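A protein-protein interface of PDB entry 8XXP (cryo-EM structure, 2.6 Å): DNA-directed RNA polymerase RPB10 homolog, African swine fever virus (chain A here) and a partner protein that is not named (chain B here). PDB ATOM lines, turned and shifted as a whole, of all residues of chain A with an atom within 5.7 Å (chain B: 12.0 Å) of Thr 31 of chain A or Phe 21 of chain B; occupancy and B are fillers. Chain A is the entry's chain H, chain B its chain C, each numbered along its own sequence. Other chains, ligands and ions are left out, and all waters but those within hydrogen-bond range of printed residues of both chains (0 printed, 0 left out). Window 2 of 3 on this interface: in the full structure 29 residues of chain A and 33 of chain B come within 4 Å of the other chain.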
ATOM      1  N   ILE A  20     -32.173   1.824  32.064  1.00  0.00           N
ATOM      2  CA  ILE A  20     -30.855   2.374  31.781  1.00  0.00           C
ATOM      3  C   ILE A  20     -30.343   1.844  30.455  1.00  0.00           C
ATOM      4  O   ILE A  20     -29.784   2.592  29.649  1.00  0.00           O
ATOM      5  CB  ILE A  20     -29.880   2.051  32.928  1.00  0.00           C
ATOM      6  CG1 ILE A  20     -30.440   2.536  34.261  1.00  0.00           C
ATOM      7  CG2 ILE A  20     -28.536   2.675  32.662  1.00  0.00           C
ATOM      8  CD1 ILE A  20     -29.746   1.945  35.455  1.00  0.00           C
ATOM      9  N   ALA A  24     -29.476   4.149  27.255  1.00  0.00           N
ATOM     10  CA  ALA A  24     -28.078   4.137  26.847  1.00  0.00           C
ATOM     11  C   ALA A  24     -27.919   3.582  25.445  1.00  0.00           C
ATOM     12  O   ALA A  24     -27.065   4.041  24.686  1.00  0.00           O
ATOM     13  CB  ALA A  24     -27.254   3.324  27.838  1.00  0.00           C
ATOM     14  N   THR A  26     -30.175   3.833  23.043  1.00  0.00           N
ATOM     15  CA  THR A  26     -30.587   4.901  22.138  1.00  0.00           C
ATOM     16  C   THR A  26     -29.455   5.900  21.923  1.00  0.00           C
ATOM     17  O   THR A  26     -29.133   6.259  20.782  1.00  0.00           O
ATOM     18  CB  THR A  26     -31.833   5.600  22.678  1.00  0.00           C
ATOM     19  OG1 THR A  26     -32.806   4.618  23.046  1.00  0.00           O
ATOM     20  CG2 THR A  26     -32.427   6.502  21.621  1.00  0.00           C
ATOM     21  N   GLU A  27     -28.810   6.331  23.012  1.00  0.00           N
ATOM     22  CA  GLU A  27     -27.708   7.284  22.865  1.00  0.00           C
ATOM     23  C   GLU A  27     -26.545   6.689  22.079  1.00  0.00           C
ATOM     24  O   GLU A  27     -25.999   7.340  21.185  1.00  0.00           O
ATOM     25  CB  GLU A  27     -27.219   7.783  24.226  1.00  0.00           C
ATOM     26  CG  GLU A  27     -28.280   7.953  25.292  1.00  0.00           C
ATOM     27  CD  GLU A  27     -29.378   8.919  24.892  1.00  0.00           C
ATOM     28  OE1 GLU A  27     -30.501   8.790  25.423  1.00  0.00           O
ATOM     29  OE2 GLU A  27     -29.119   9.817  24.060  1.00  0.00           O
ATOM     30  N   TYR A  28     -26.159   5.452  22.386  1.00  0.00           N
ATOM     31  CA  TYR A  28     -24.976   4.869  21.762  1.00  0.00           C
ATOM     32  C   TYR A  28     -25.222   4.573  20.288  1.00  0.00           C
ATOM     33  O   TYR A  28     -24.295   4.639  19.474  1.00  0.00           O
ATOM     34  CB  TYR A  28     -24.557   3.618  22.538  1.00  0.00           C
ATOM     35  CG  TYR A  28     -23.560   2.699  21.858  1.00  0.00           C
ATOM     36  CD1 TYR A  28     -22.241   2.660  22.279  1.00  0.00           C
ATOM     37  CD2 TYR A  28     -23.950   1.816  20.860  1.00  0.00           C
ATOM     38  CE1 TYR A  28     -21.328   1.816  21.688  1.00  0.00           C
ATOM     39  CE2 TYR A  28     -23.046   0.974  20.267  1.00  0.00           C
ATOM     40  CZ  TYR A  28     -21.737   0.973  20.684  1.00  0.00           C
ATOM     41  OH  TYR A  28     -20.835   0.122  20.089  1.00  0.00           O
ATOM     42  N   ILE A  29     -26.460   4.234  19.927  1.00  0.00           N
ATOM     43  CA  ILE A  29     -26.815   4.128  18.517  1.00  0.00           C
ATOM     44  C   ILE A  29     -26.728   5.494  17.852  1.00  0.00           C
ATOM     45  O   ILE A  29     -26.218   5.623  16.733  1.00  0.00           O
ATOM     46  CB  ILE A  29     -28.217   3.511  18.356  1.00  0.00           C
ATOM     47  CG1 ILE A  29     -28.237   2.046  18.793  1.00  0.00           C
ATOM     48  CG2 ILE A  29     -28.689   3.623  16.922  1.00  0.00           C
ATOM     49  CD1 ILE A  29     -26.970   1.293  18.516  1.00  0.00           C
ATOM     50  N   LYS A  30     -27.214   6.537  18.533  1.00  0.00           N
ATOM     51  CA  LYS A  30     -27.231   7.862  17.919  1.00  0.00           C
ATOM     52  C   LYS A  30     -25.822   8.370  17.631  1.00  0.00           C
ATOM     53  O   LYS A  30     -25.623   9.128  16.676  1.00  0.00           O
ATOM     54  CB  LYS A  30     -28.017   8.834  18.805  1.00  0.00           C
ATOM     55  CG  LYS A  30     -27.565  10.285  18.782  1.00  0.00           C
ATOM     56  CD  LYS A  30     -27.743  10.957  20.138  1.00  0.00           C
ATOM     57  CE  LYS A  30     -26.725  10.495  21.163  1.00  0.00           C
ATOM     58  NZ  LYS A  30     -25.340  10.848  20.765  1.00  0.00           N
ATOM     59  N   THR A  31     -24.828   7.944  18.416  1.00  0.00           N
ATOM     60  CA  THR A  31     -23.449   8.297  18.083  1.00  0.00           C
ATOM     61  C   THR A  31     -22.938   7.486  16.900  1.00  0.00           C
ATOM     62  O   THR A  31     -22.276   8.028  16.009  1.00  0.00           O
ATOM     63  CB  THR A  31     -22.524   8.085  19.281  1.00  0.00           C
ATOM     64  OG1 THR A  31     -22.186   6.699  19.386  1.00  0.00           O
ATOM     65  CG2 THR A  31     -23.186   8.532  20.556  1.00  0.00           C
ATOM     66  N   LYS A  32     -23.232   6.185  16.878  1.00  0.00           N
ATOM     67  CA  LYS A  32     -22.617   5.294  15.897  1.00  0.00           C
ATOM     68  C   LYS A  32     -23.060   5.628  14.478  1.00  0.00           C
ATOM     69  O   LYS A  32     -22.237   5.674  13.559  1.00  0.00           O
ATOM     70  CB  LYS A  32     -22.943   3.841  16.234  1.00  0.00           C
ATOM     71  CG  LYS A  32     -22.165   3.296  17.410  1.00  0.00           C
ATOM     72  CD  LYS A  32     -20.766   2.882  16.999  1.00  0.00           C
ATOM     73  CE  LYS A  32     -19.845   2.790  18.202  1.00  0.00           C
ATOM     74  NZ  LYS A  32     -19.954   3.987  19.076  1.00  0.00           N
ATOM     75  N   MET A  33     -24.352   5.858  14.278  1.00  0.00           N
ATOM     76  CA  MET A  33     -24.855   6.166  12.945  1.00  0.00           C
ATOM     77  C   MET A  33     -25.241   7.636  12.828  1.00  0.00           C
ATOM     78  O   MET A  33     -24.493   8.438  12.268  1.00  0.00           O
ATOM     79  CB  MET A  33     -26.050   5.277  12.597  1.00  0.00           C
ATOM     80  CG  MET A  33     -26.963   4.969  13.767  1.00  0.00           C
ATOM     81  SD  MET A  33     -28.693   4.823  13.288  1.00  0.00           S
ATOM     82  CE  MET A  33     -29.027   6.483  12.707  1.00  0.00           C
ATOM     83  N   LEU A  54     -21.941  -2.419  25.950  1.00  0.00           N
ATOM     84  CA  LEU A  54     -22.963  -1.681  26.686  1.00  0.00           C
ATOM     85  C   LEU A  54     -23.635  -2.554  27.737  1.00  0.00           C
ATOM     86  O   LEU A  54     -23.874  -2.109  28.864  1.00  0.00           O
ATOM     87  CB  LEU A  54     -24.011  -1.135  25.722  1.00  0.00           C
ATOM     88  CG  LEU A  54     -24.047   0.363  25.466  1.00  0.00           C
ATOM     89  CD1 LEU A  54     -25.258   0.692  24.624  1.00  0.00           C
ATOM     90  CD2 LEU A  54     -24.080   1.120  26.772  1.00  0.00           C
ATOM     91  N   ILE B  15     -22.547  -2.158  38.292  1.00  0.00           N
ATOM     92  CA  ILE B  15     -22.678  -1.287  37.131  1.00  0.00           C
ATOM     93  C   ILE B  15     -21.359  -0.568  36.902  1.00  0.00           C
ATOM     94  O   ILE B  15     -20.730  -0.085  37.850  1.00  0.00           O
ATOM     95  CB  ILE B  15     -23.822  -0.287  37.336  1.00  0.00           C
ATOM     96  CG1 ILE B  15     -25.097  -1.021  37.743  1.00  0.00           C
ATOM     97  CG2 ILE B  15     -24.056   0.505  36.079  1.00  0.00           C
ATOM     98  CD1 ILE B  15     -26.173  -0.117  38.286  1.00  0.00           C
ATOM     99  N   ASP B  16     -20.929  -0.503  35.649  1.00  0.00           N
ATOM    100  CA  ASP B  16     -19.681   0.168  35.295  1.00  0.00           C
ATOM    101  C   ASP B  16     -20.005   1.578  34.821  1.00  0.00           C
ATOM    102  O   ASP B  16     -20.405   1.784  33.674  1.00  0.00           O
ATOM    103  CB  ASP B  16     -18.929  -0.618  34.233  1.00  0.00           C
ATOM    104  CG  ASP B  16     -17.476  -0.232  34.152  1.00  0.00           C
ATOM    105  OD1 ASP B  16     -16.983   0.421  35.095  1.00  0.00           O
ATOM    106  OD2 ASP B  16     -16.826  -0.572  33.143  1.00  0.00           O
ATOM    107  N   PHE B  17     -19.820   2.556  35.703  1.00  0.00           N
ATOM    108  CA  PHE B  17     -20.054   3.952  35.364  1.00  0.00           C
ATOM    109  C   PHE B  17     -18.904   4.563  34.577  1.00  0.00           C
ATOM    110  O   PHE B  17     -19.003   5.720  34.157  1.00  0.00           O
ATOM    111  CB  PHE B  17     -20.319   4.757  36.634  1.00  0.00           C
ATOM    112  CG  PHE B  17     -21.640   4.451  37.273  1.00  0.00           C
ATOM    113  CD1 PHE B  17     -22.816   4.931  36.727  1.00  0.00           C
ATOM    114  CD2 PHE B  17     -21.708   3.672  38.414  1.00  0.00           C
ATOM    115  CE1 PHE B  17     -24.032   4.645  37.310  1.00  0.00           C
ATOM    116  CE2 PHE B  17     -22.920   3.386  39.002  1.00  0.00           C
ATOM    117  CZ  PHE B  17     -24.084   3.871  38.450  1.00  0.00           C
ATOM    118  N   SER B  18     -17.817   3.819  34.370  1.00  0.00           N
ATOM    119  CA  SER B  18     -16.798   4.244  33.423  1.00  0.00           C
ATOM    120  C   SER B  18     -17.331   4.269  32.000  1.00  0.00           C
ATOM    121  O   SER B  18     -16.698   4.862  31.121  1.00  0.00           O
ATOM    122  CB  SER B  18     -15.582   3.325  33.511  1.00  0.00           C
ATOM    123  OG  SER B  18     -14.690   3.758  34.520  1.00  0.00           O
ATOM    124  N   ASN B  19     -18.463   3.621  31.752  1.00  0.00           N
ATOM    125  CA  ASN B  19     -19.147   3.720  30.472  1.00  0.00           C
ATOM    126  C   ASN B  19     -19.936   5.018  30.445  1.00  0.00           C
ATOM    127  O   ASN B  19     -20.805   5.239  31.292  1.00  0.00           O
ATOM    128  CB  ASN B  19     -20.063   2.517  30.266  1.00  0.00           C
ATOM    129  CG  ASN B  19     -20.485   2.342  28.821  1.00  0.00           C
ATOM    130  OD1 ASN B  19     -21.214   3.162  28.276  1.00  0.00           O
ATOM    131  ND2 ASN B  19     -20.022   1.272  28.195  1.00  0.00           N
ATOM    132  N   LEU B  20     -19.626   5.884  29.480  1.00  0.00           N
ATOM    133  CA  LEU B  20     -20.263   7.194  29.441  1.00  0.00           C
ATOM    134  C   LEU B  20     -21.766   7.072  29.245  1.00  0.00           C
ATOM    135  O   LEU B  20     -22.541   7.782  29.892  1.00  0.00           O
ATOM    136  CB  LEU B  20     -19.645   8.047  28.333  1.00  0.00           C
ATOM    137  CG  LEU B  20     -18.495   8.984  28.715  1.00  0.00           C
ATOM    138  CD1 LEU B  20     -17.550   8.348  29.723  1.00  0.00           C
ATOM    139  CD2 LEU B  20     -17.736   9.416  27.475  1.00  0.00           C
ATOM    140  N   PHE B  21     -22.197   6.177  28.359  1.00  0.00           N
ATOM    141  CA  PHE B  21     -23.619   6.051  28.069  1.00  0.00           C
ATOM    142  C   PHE B  21     -24.387   5.525  29.271  1.00  0.00           C
ATOM    143  O   PHE B  21     -25.481   6.010  29.570  1.00  0.00           O
ATOM    144  CB  PHE B  21     -23.819   5.155  26.854  1.00  0.00           C
ATOM    145  CG  PHE B  21     -23.034   5.593  25.666  1.00  0.00           C
ATOM    146  CD1 PHE B  21     -23.524   6.571  24.826  1.00  0.00           C
ATOM    147  CD2 PHE B  21     -21.794   5.055  25.405  1.00  0.00           C
ATOM    148  CE1 PHE B  21     -22.800   6.986  23.741  1.00  0.00           C
ATOM    149  CE2 PHE B  21     -21.067   5.469  24.322  1.00  0.00           C
ATOM    150  CZ  PHE B  21     -21.571   6.436  23.488  1.00  0.00           C
ATOM    151  N   ILE B  22     -23.827   4.546  29.978  1.00  0.00           N
ATOM    152  CA  ILE B  22     -24.498   4.010  31.157  1.00  0.00           C
ATOM    153  C   ILE B  22     -24.615   5.080  32.233  1.00  0.00           C
ATOM    154  O   ILE B  22     -25.670   5.247  32.858  1.00  0.00           O
ATOM    155  CB  ILE B  22     -23.760   2.766  31.681  1.00  0.00           C
ATOM    156  CG1 ILE B  22     -23.862   1.624  30.673  1.00  0.00           C
ATOM    157  CG2 ILE B  22     -24.325   2.345  33.017  1.00  0.00           C
ATOM    158  CD1 ILE B  22     -25.263   1.350  30.223  1.00  0.00           C
ATOM    159  N   LYS B  23     -23.528   5.819  32.471  1.00  0.00           N
ATOM    160  CA  LYS B  23     -23.554   6.856  33.496  1.00  0.00           C
ATOM    161  C   LYS B  23     -24.543   7.955  33.143  1.00  0.00           C
ATOM    162  O   LYS B  23     -25.327   8.392  33.994  1.00  0.00           O
ATOM    163  CB  LYS B  23     -22.155   7.433  33.695  1.00  0.00           C
ATOM    164  CG  LYS B  23     -21.952   8.062  35.058  1.00  0.00           C
ATOM    165  CD  LYS B  23     -20.486   8.272  35.367  1.00  0.00           C
ATOM    166  CE  LYS B  23     -20.314   9.206  36.549  1.00  0.00           C
ATOM    167  NZ  LYS B  23     -21.628   9.618  37.113  1.00  0.00           N
ATOM    168  N   ASN B  24     -24.534   8.401  31.886  1.00  0.00           N
ATOM    169  CA  ASN B  24     -25.475   9.428  31.460  1.00  0.00           C
ATOM    170  C   ASN B  24     -26.911   8.949  31.600  1.00  0.00           C
ATOM    171  O   ASN B  24     -27.771   9.688  32.088  1.00  0.00           O
ATOM    172  CB  ASN B  24     -25.198   9.836  30.015  1.00  0.00           C
ATOM    173  CG  ASN B  24     -23.911  10.602  29.862  1.00  0.00           C
ATOM    174  OD1 ASN B  24     -23.299  11.009  30.845  1.00  0.00           O
ATOM    175  ND2 ASN B  24     -23.489  10.804  28.624  1.00  0.00           N
ATOM    176  N   ALA B  25     -27.192   7.714  31.177  1.00  0.00           N
ATOM    177  CA  ALA B  25     -28.557   7.208  31.239  1.00  0.00           C
ATOM    178  C   ALA B  25     -29.034   7.073  32.674  1.00  0.00           C
ATOM    179  O   ALA B  25     -30.160   7.465  32.998  1.00  0.00           O
ATOM    180  CB  ALA B  25     -28.647   5.867  30.515  1.00  0.00           C
ATOM    181  N   ALA B  26     -28.192   6.521  33.551  1.00  0.00           N
ATOM    182  CA  ALA B  26     -28.576   6.370  34.949  1.00  0.00           C
ATOM    183  C   ALA B  26     -28.794   7.723  35.607  1.00  0.00           C
ATOM    184  O   ALA B  26     -29.743   7.898  36.378  1.00  0.00           O
ATOM    185  CB  ALA B  26     -27.519   5.567  35.701  1.00  0.00           C
ATOM    186  N   LYS B  27     -27.930   8.697  35.308  1.00  0.00           N
ATOM    187  CA  LYS B  27     -28.104  10.034  35.863  1.00  0.00           C
ATOM    188  C   LYS B  27     -29.386  10.686  35.357  1.00  0.00           C
ATOM    189  O   LYS B  27     -30.120  11.303  36.135  1.00  0.00           O
ATOM    190  CB  LYS B  27     -26.882  10.892  35.534  1.00  0.00           C
ATOM    191  CG  LYS B  27     -27.186  12.306  35.090  1.00  0.00           C
ATOM    192  CD  LYS B  27     -25.923  13.158  35.035  1.00  0.00           C
ATOM    193  CE  LYS B  27     -25.040  12.789  33.848  1.00  0.00           C
ATOM    194  NZ  LYS B  27     -25.600  13.254  32.545  1.00  0.00           N
ATOM    195  N   LYS B  28     -29.690  10.540  34.067  1.00  0.00           N
ATOM    196  CA  LYS B  28     -30.857  11.214  33.511  1.00  0.00           C
ATOM    197  C   LYS B  28     -32.152  10.562  33.972  1.00  0.00           C
ATOM    198  O   LYS B  28     -33.178  11.238  34.099  1.00  0.00           O
ATOM    199  CB  LYS B  28     -30.787  11.232  31.985  1.00  0.00           C
ATOM    200  CG  LYS B  28     -29.695  12.121  31.394  1.00  0.00           C
ATOM    201  CD  LYS B  28     -29.288  13.259  32.321  1.00  0.00           C
ATOM    202  CE  LYS B  28     -30.186  14.477  32.165  1.00  0.00           C
ATOM    203  NZ  LYS B  28     -30.221  15.290  33.409  1.00  0.00           N
ATOM    204  N   LEU B  29     -32.133   9.253  34.223  1.00  0.00           N
ATOM    205  CA  LEU B  29     -33.348   8.539  34.600  1.00  0.00           C
ATOM    206  C   LEU B  29     -33.575   8.533  36.108  1.00  0.00           C
ATOM    207  O   LEU B  29     -34.623   8.975  36.584  1.00  0.00           O
ATOM    208  CB  LEU B  29     -33.298   7.104  34.068  1.00  0.00           C
ATOM    209  CG  LEU B  29     -33.463   6.921  32.560  1.00  0.00           C
ATOM    210  CD1 LEU B  29     -33.241   5.472  32.184  1.00  0.00           C
ATOM    211  CD2 LEU B  29     -34.835   7.384  32.111  1.00  0.00           C
ATOM    212  N   PHE B  30     -32.611   8.024  36.869  1.00  0.00           N
ATOM    213  CA  PHE B  30     -32.799   7.792  38.293  1.00  0.00           C
ATOM    214  C   PHE B  30     -31.901   8.649  39.168  1.00  0.00           C
ATOM    215  O   PHE B  30     -31.911   8.473  40.391  1.00  0.00           O
ATOM    216  CB  PHE B  30     -32.562   6.309  38.616  1.00  0.00           C
ATOM    217  CG  PHE B  30     -33.325   5.371  37.731  1.00  0.00           C
ATOM    218  CD1 PHE B  30     -34.674   5.155  37.931  1.00  0.00           C
ATOM    219  CD2 PHE B  30     -32.699   4.729  36.681  1.00  0.00           C
ATOM    220  CE1 PHE B  30     -35.377   4.308  37.113  1.00  0.00           C
ATOM    221  CE2 PHE B  30     -33.400   3.883  35.860  1.00  0.00           C
ATOM    222  CZ  PHE B  30     -34.738   3.672  36.074  1.00  0.00           C
ATOM    223  N   GLN B  31     -31.134   9.570  38.581  1.00  0.00           N
ATOM    224  CA  GLN B  31     -30.122  10.329  39.315  1.00  0.00           C
ATOM    225  C   GLN B  31     -29.168   9.382  40.035  1.00  0.00           C
ATOM    226  O   GLN B  31     -28.779   9.602  41.183  1.00  0.00           O
ATOM    227  CB  GLN B  31     -30.765  11.313  40.294  1.00  0.00           C
ATOM    228  CG  GLN B  31     -31.326  12.561  39.648  1.00  0.00           C
ATOM    229  CD  GLN B  31     -32.621  12.304  38.907  1.00  0.00           C
ATOM    230  OE1 GLN B  31     -33.597  11.831  39.488  1.00  0.00           O
ATOM    231  NE2 GLN B  31     -32.637  12.623  37.619  1.00  0.00           N
ATOM    232  N   LEU B  32     -28.799   8.308  39.348  1.00  0.00           N
ATOM    233  CA  LEU B  32     -27.997   7.236  39.921  1.00  0.00           C
ATOM    234  C   LEU B  32     -26.547   7.450  39.508  1.00  0.00           C
ATOM    235  O   LEU B  32     -26.195   7.296  38.335  1.00  0.00           O
ATOM    236  CB  LEU B  32     -28.516   5.876  39.462  1.00  0.00           C
ATOM    237  CG  LEU B  32     -27.863   4.619  40.034  1.00  0.00           C
ATOM    238  CD1 LEU B  32     -28.365   4.343  41.431  1.00  0.00           C
ATOM    239  CD2 LEU B  32     -28.135   3.435  39.131  1.00  0.00           C
ATOM    240  N   GLU B  33     -25.714   7.825  40.473  1.00  0.00           N
ATOM    241  CA  GLU B  33     -24.288   8.001  40.260  1.00  0.00           C
ATOM    242  C   GLU B  33     -23.468   6.889  40.890  1.00  0.00           C
ATOM    243  O   GLU B  33     -22.247   6.863  40.720  1.00  0.00           O
ATOM    244  CB  GLU B  33     -23.833   9.350  40.820  1.00  0.00           C
ATOM    245  CG  GLU B  33     -24.756  10.519  40.504  1.00  0.00           C
ATOM    246  CD  GLU B  33     -24.698  10.936  39.053  1.00  0.00           C
ATOM    247  OE1 GLU B  33     -23.658  10.695  38.406  1.00  0.00           O
ATOM    248  OE2 GLU B  33     -25.689  11.511  38.559  1.00  0.00           O
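Printed residues of chain B that touch a printed residue of chain A: Asn 19, Phe 21, Ile 22, Ala 25, Ala 26, Leu 29 and Phe 30.
Hydrophobic or aromatic side chains of chain B within 4 Å of the printed part of chain A: Phe 21, Ile 22, Ala 25, Leu 29 and Phe 30.
Along chain B the printed residues that touch a printed residue of chain A span positions 19 to 30.
Hydrophobic or aromatic side chains of chain A that line the printed part of chain B: Ile 20, Ala 24, Tyr 28 and Leu 54.
Among the printed residues, no Asp or Glu carboxylate lies within 4 Å of a Lys or Arg side-chain nitrogen of the other chain.
Among the printed residues, merely in contact across the chains: Thr 31 of chain A with Phe 21 of chain B (3.6 Å), Ile 20 of chain A with Ala 25 of chain B (3.6 Å), Ile 20 of chain A with Phe 30 of chain B (3.6 Å), Tyr 28 of chain A with Phe 21 of chain B (3.6 Å), Ala 24 of chain A with Phe 21 of chain B (3.7 Å), Leu 54 of chain A with Ile 22 of chain B (3.7 Å), Ala 24 of chain A with Ile 22 of chain B (3.7 Å), Ala 24 of chain A with Ala 25 of chain B (3.8 Å), Ile 20 of chain A with Leu 29 of chain B (3.8 Å), Leu 54 of chain A with Asn 19 of chain B (3.8 Å), Ile 20 of chain A with Ile 22 of chain B (3.9 Å), Glu 27 of chain A with Phe 21 of chain B (3.9 Å) and Ile 20 of chain A with Ala 26 of chain B (3.96 Å).
Thr 31 of chain A touches just one residue of chain B: Phe 21 (3.6 Å).
Glu 27 of chain A touches one residue of chain B.
Tyr 28 of chain A touches one residue of chain B.
Lys 30 of chain A touches none of the printed residues of chain B.
Met 33 of chain A touches none of the printed residues of chain B.
Of chain B, only Asn 19 and Ile 22 come within 4 Å of Leu 54 of chain A.
Printed residues of chain A within 4 Å of Asn 19 of chain B: Leu 54 (3.8 Å).
Of the printed residues of chain A, Ala 26 of chain B touches Ile 20 (3.96 Å).
Printed residues of chain A within 4 Å of Leu 29 of chain B: Ile 20.
Of the printed residues of chain A, Phe 30 of chain B touches Ile 20 (3.6 Å).
Printed residues of chain B within 4 Å of Ile 20 of chain A: Ile 22 (3.9 Å), Ala 25 (3.6 Å), Ala 26 (3.96 Å), Leu 29 (3.8 Å) and Phe 30 (3.6 Å).
The nearest printed residue of chain A that does not touch Ala 25 of chain B is Glu 27 of chain A (5.6 Å).
The backbone NH (N) of Ile 22 of chain B sits at hydrogen-bond distance from the side-chain amide oxygen (OD1) of Asn 19 of chain B, at 3.4 Å.
The backbone NH of Gln 31 of chain B sits at hydrogen-bond distance from the backbone carbonyl oxygen of Ala 26 of chain B (3.1 Å).
The side-chain amide oxygen (OD1) of Asn 19 of chain B lies within hydrogen-bond range of the backbone NH (N) of Phe 21 of chain B.
O of Tyr 28 of chain A lies within hydrogen-bond range of OG1 of Thr 31 of chain A, 2.9 Å away.
N of Leu 32 of chain B is in hydrogen-bond range of O of Ala 26 of chain B (3.1 Å).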
